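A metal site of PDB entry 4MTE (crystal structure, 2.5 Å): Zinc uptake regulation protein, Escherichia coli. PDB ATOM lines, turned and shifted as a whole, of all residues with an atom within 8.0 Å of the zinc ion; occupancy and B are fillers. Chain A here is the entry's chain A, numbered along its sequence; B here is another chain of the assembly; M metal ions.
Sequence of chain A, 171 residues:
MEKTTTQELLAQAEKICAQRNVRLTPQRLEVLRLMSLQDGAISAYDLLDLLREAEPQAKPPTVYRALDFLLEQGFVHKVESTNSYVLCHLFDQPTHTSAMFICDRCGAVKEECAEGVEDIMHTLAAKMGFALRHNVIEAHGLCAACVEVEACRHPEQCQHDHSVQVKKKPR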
ATOM      1  N   ILE A 102      -1.142 -11.628 -10.859  1.00  0.00           N
ATOM      2  CA  ILE A 102      -1.211 -10.283 -11.393  1.00  0.00           C
ATOM      3  C   ILE A 102      -2.467  -9.567 -10.909  1.00  0.00           C
ATOM      4  O   ILE A 102      -3.584 -10.025 -11.152  1.00  0.00           O
ATOM      5  CB  ILE A 102      -1.242 -10.301 -12.936  1.00  0.00           C
ATOM      6  CG1 ILE A 102      -0.096 -11.141 -13.492  1.00  0.00           C
ATOM      7  CG2 ILE A 102      -1.179  -8.875 -13.492  1.00  0.00           C
ATOM      8  CD1 ILE A 102      -0.316 -11.597 -14.919  1.00  0.00           C
ATOM      9  N   CYS A 103      -2.286  -8.433 -10.249  1.00  0.00           N
ATOM     10  CA  CYS A 103      -3.410  -7.608  -9.854  1.00  0.00           C
ATOM     11  C   CYS A 103      -3.933  -6.834 -11.050  1.00  0.00           C
ATOM     12  O   CYS A 103      -3.201  -6.059 -11.669  1.00  0.00           O
ATOM     13  CB  CYS A 103      -3.008  -6.636  -8.739  1.00  0.00           C
ATOM     14  SG  CYS A 103      -4.352  -5.539  -8.239  1.00  0.00           S
ATOM     15  N   ASP A 104      -5.207  -7.030 -11.387  1.00  0.00           N
ATOM     16  CA  ASP A 104      -5.826  -6.369 -12.531  1.00  0.00           C
ATOM     17  C   ASP A 104      -6.094  -4.895 -12.255  1.00  0.00           C
ATOM     18  O   ASP A 104      -6.510  -4.155 -13.155  1.00  0.00           O
ATOM     19  CB  ASP A 104      -7.131  -7.066 -12.912  1.00  0.00           C
ATOM     20  CG  ASP A 104      -6.919  -8.469 -13.451  1.00  0.00           C
ATOM     21  OD1 ASP A 104      -5.858  -8.720 -14.064  1.00  0.00           O
ATOM     22  OD2 ASP A 104      -7.817  -9.313 -13.266  1.00  0.00           O
ATOM     23  N   ARG A 105      -5.871  -4.459 -11.013  1.00  0.00           N
ATOM     24  CA  ARG A 105      -6.132  -3.088 -10.617  1.00  0.00           C
ATOM     25  C   ARG A 105      -4.872  -2.222 -10.573  1.00  0.00           C
ATOM     26  O   ARG A 105      -4.835  -1.149 -11.175  1.00  0.00           O
ATOM     27  CB  ARG A 105      -6.818  -3.049  -9.249  1.00  0.00           C
ATOM     28  CG  ARG A 105      -7.006  -1.644  -8.713  1.00  0.00           C
ATOM     29  CD  ARG A 105      -8.000  -1.583  -7.576  1.00  0.00           C
ATOM     30  NE  ARG A 105      -8.226  -0.211  -7.130  1.00  0.00           N
ATOM     31  CZ  ARG A 105      -7.432   0.442  -6.286  1.00  0.00           C
ATOM     32  NH1 ARG A 105      -6.339  -0.140  -5.803  1.00  0.00           N
ATOM     33  NH2 ARG A 105      -7.714   1.691  -5.945  1.00  0.00           N
ATOM     34  N   CYS A 106      -3.846  -2.674  -9.856  1.00  0.00           N
ATOM     35  CA  CYS A 106      -2.648  -1.873  -9.628  1.00  0.00           C
ATOM     36  C   CYS A 106      -1.475  -2.303 -10.513  1.00  0.00           C
ATOM     37  O   CYS A 106      -0.467  -1.588 -10.598  1.00  0.00           O
ATOM     38  CB  CYS A 106      -2.227  -1.941  -8.158  1.00  0.00           C
ATOM     39  SG  CYS A 106      -1.532  -3.528  -7.658  1.00  0.00           S
ATOM     40  N   GLY A 107      -1.585  -3.460 -11.150  1.00  0.00           N
ATOM     41  CA  GLY A 107      -0.549  -3.938 -12.040  1.00  0.00           C
ATOM     42  C   GLY A 107       0.573  -4.668 -11.326  1.00  0.00           C
ATOM     43  O   GLY A 107       1.542  -5.089 -11.959  1.00  0.00           O
ATOM     44  N   ALA A 108       0.445  -4.816 -10.011  1.00  0.00           N
ATOM     45  CA  ALA A 108       1.463  -5.506  -9.211  1.00  0.00           C
ATOM     46  C   ALA A 108       1.519  -6.975  -9.590  1.00  0.00           C
ATOM     47  O   ALA A 108       0.516  -7.556 -10.024  1.00  0.00           O
ATOM     48  CB  ALA A 108       1.187  -5.351  -7.724  1.00  0.00           C
ATOM     49  N   VAL A 109       2.693  -7.589  -9.429  1.00  0.00           N
ATOM     50  CA  VAL A 109       2.902  -8.974  -9.818  1.00  0.00           C
ATOM     51  C   VAL A 109       3.687  -9.707  -8.745  1.00  0.00           C
ATOM     52  O   VAL A 109       4.786  -9.289  -8.377  1.00  0.00           O
ATOM     53  CB  VAL A 109       3.663  -9.069 -11.160  1.00  0.00           C
ATOM     54  CG1 VAL A 109       3.907 -10.530 -11.549  1.00  0.00           C
ATOM     55  CG2 VAL A 109       2.896  -8.343 -12.258  1.00  0.00           C
ATOM     56  N   GLY A 141      -6.388 -11.355 -10.880  1.00  0.00           N
ATOM     57  CA  GLY A 141      -7.196 -11.145  -9.704  1.00  0.00           C
ATOM     58  C   GLY A 141      -6.820  -9.835  -9.029  1.00  0.00           C
ATOM     59  O   GLY A 141      -6.541  -8.850  -9.693  1.00  0.00           O
ATOM     60  N   LEU A 142      -6.809  -9.851  -7.695  1.00  0.00           N
ATOM     61  CA  LEU A 142      -6.508  -8.668  -6.911  1.00  0.00           C
ATOM     62  C   LEU A 142      -5.533  -8.988  -5.791  1.00  0.00           C
ATOM     63  O   LEU A 142      -5.668 -10.024  -5.132  1.00  0.00           O
ATOM     64  CB  LEU A 142      -7.789  -8.087  -6.315  1.00  0.00           C
ATOM     65  CG  LEU A 142      -8.802  -7.492  -7.291  1.00  0.00           C
ATOM     66  CD1 LEU A 142      -9.733  -8.561  -7.868  1.00  0.00           C
ATOM     67  CD2 LEU A 142      -9.593  -6.399  -6.605  1.00  0.00           C
ATOM     68  N   CYS A 143      -4.561  -8.120  -5.575  1.00  0.00           N
ATOM     69  CA  CYS A 143      -3.644  -8.271  -4.448  1.00  0.00           C
ATOM     70  C   CYS A 143      -4.365  -7.853  -3.170  1.00  0.00           C
ATOM     71  O   CYS A 143      -5.443  -7.267  -3.218  1.00  0.00           O
ATOM     72  CB  CYS A 143      -2.375  -7.451  -4.657  1.00  0.00           C
ATOM     73  SG  CYS A 143      -2.619  -5.660  -4.665  1.00  0.00           S
ATOM     74  N   ALA A 144      -3.738  -8.157  -2.028  1.00  0.00           N
ATOM     75  CA  ALA A 144      -4.324  -7.880  -0.718  1.00  0.00           C
ATOM     76  C   ALA A 144      -4.798  -6.435  -0.556  1.00  0.00           C
ATOM     77  O   ALA A 144      -5.950  -6.195  -0.174  1.00  0.00           O
ATOM     78  CB  ALA A 144      -3.298  -8.209   0.368  1.00  0.00           C
ATOM     79  N   ALA A 145      -3.910  -5.486  -0.848  1.00  0.00           N
ATOM     80  CA  ALA A 145      -4.226  -4.066  -0.720  1.00  0.00           C
ATOM     81  C   ALA A 145      -5.461  -3.727  -1.563  1.00  0.00           C
ATOM     82  O   ALA A 145      -6.455  -3.186  -1.048  1.00  0.00           O
ATOM     83  CB  ALA A 145      -3.046  -3.226  -1.157  1.00  0.00           C
ATOM     84  N   CYS A 146      -5.395  -4.053  -2.837  1.00  0.00           N
ATOM     85  CA  CYS A 146      -6.482  -3.780  -3.763  1.00  0.00           C
ATOM     86  C   CYS A 146      -7.750  -4.537  -3.350  1.00  0.00           C
ATOM     87  O   CYS A 146      -8.866  -4.120  -3.668  1.00  0.00           O
ATOM     88  CB  CYS A 146      -6.087  -4.155  -5.197  1.00  0.00           C
ATOM     89  SG  CYS A 146      -4.929  -2.995  -5.983  1.00  0.00           S
ATOM     90  N   VAL A 147      -7.571  -5.637  -2.628  1.00  0.00           N
ATOM     91  CA  VAL A 147      -8.704  -6.393  -2.097  1.00  0.00           C
ATOM     92  C   VAL A 147      -9.364  -5.601  -0.973  1.00  0.00           C
ATOM     93  O   VAL A 147     -10.582  -5.429  -0.956  1.00  0.00           O
ATOM     94  CB  VAL A 147      -8.293  -7.808  -1.602  1.00  0.00           C
ATOM     95  CG1 VAL A 147      -9.218  -8.323  -0.490  1.00  0.00           C
ATOM     96  CG2 VAL A 147      -8.245  -8.790  -2.765  1.00  0.00           C
ATOM     97  N   VAL A 149      -9.131  -2.461  -0.544  1.00  0.00           N
ATOM     98  CA  VAL A 149      -9.670  -1.263  -1.176  1.00  0.00           C
ATOM     99  C   VAL A 149     -11.036  -1.515  -1.812  1.00  0.00           C
ATOM    100  O   VAL A 149     -11.930  -0.669  -1.739  1.00  0.00           O
ATOM    101  CB  VAL A 149      -8.693  -0.700  -2.240  1.00  0.00           C
ATOM    102  CG1 VAL A 149      -9.380   0.348  -3.128  1.00  0.00           C
ATOM    103  CG2 VAL A 149      -7.457  -0.114  -1.570  1.00  0.00           C
ATOM    104  N   PHE B 130      -4.222 -12.756  -1.967  1.00  0.00           N
ATOM    105  CA  PHE B 130      -4.561 -12.566  -3.384  1.00  0.00           C
ATOM    106  C   PHE B 130      -5.896 -13.199  -3.771  1.00  0.00           C
ATOM    107  O   PHE B 130      -6.049 -14.419  -3.781  1.00  0.00           O
ATOM    108  CB  PHE B 130      -3.449 -13.113  -4.275  1.00  0.00           C
ATOM    109  CG  PHE B 130      -3.550 -12.689  -5.719  1.00  0.00           C
ATOM    110  CD1 PHE B 130      -2.920 -11.540  -6.158  1.00  0.00           C
ATOM    111  CD2 PHE B 130      -4.273 -13.444  -6.626  1.00  0.00           C
ATOM    112  CE1 PHE B 130      -3.019 -11.143  -7.476  1.00  0.00           C
ATOM    113  CE2 PHE B 130      -4.377 -13.045  -7.952  1.00  0.00           C
ATOM    114  CZ  PHE B 130      -3.742 -11.887  -8.369  1.00  0.00           C
HETATM  115 ZN    ZN M   1      -3.304  -4.542  -6.514  1.00  0.00          ZN
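The zinc ion is bound by SG of Cys 103 (2.3 Å), SG of Cys 143 (2.3 Å), SG of Cys 146 (2.3 Å) and SG of Cys 106 (2.3 Å).
The zinc ion has four donor atoms within binding distance.
Within 4 Å of the zinc ion: Cys 103, Cys 106, Cys 143 and Cys 146.
The backbone NH of Arg 105 sits close to the side-chain sulfur of Cys 103 (3.3 Å).
N of Ala 108 sits close to SG of Cys 106 (3.3 Å).
The backbone carbonyl oxygen (O) of Ala 108 is in hydrogen-bond range of the backbone NH (N) of Cys 103 (2.9 Å).
The side-chain sulfur of Cys 146 sits close to the guanidinium group of Arg 105 (3.2 Å).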
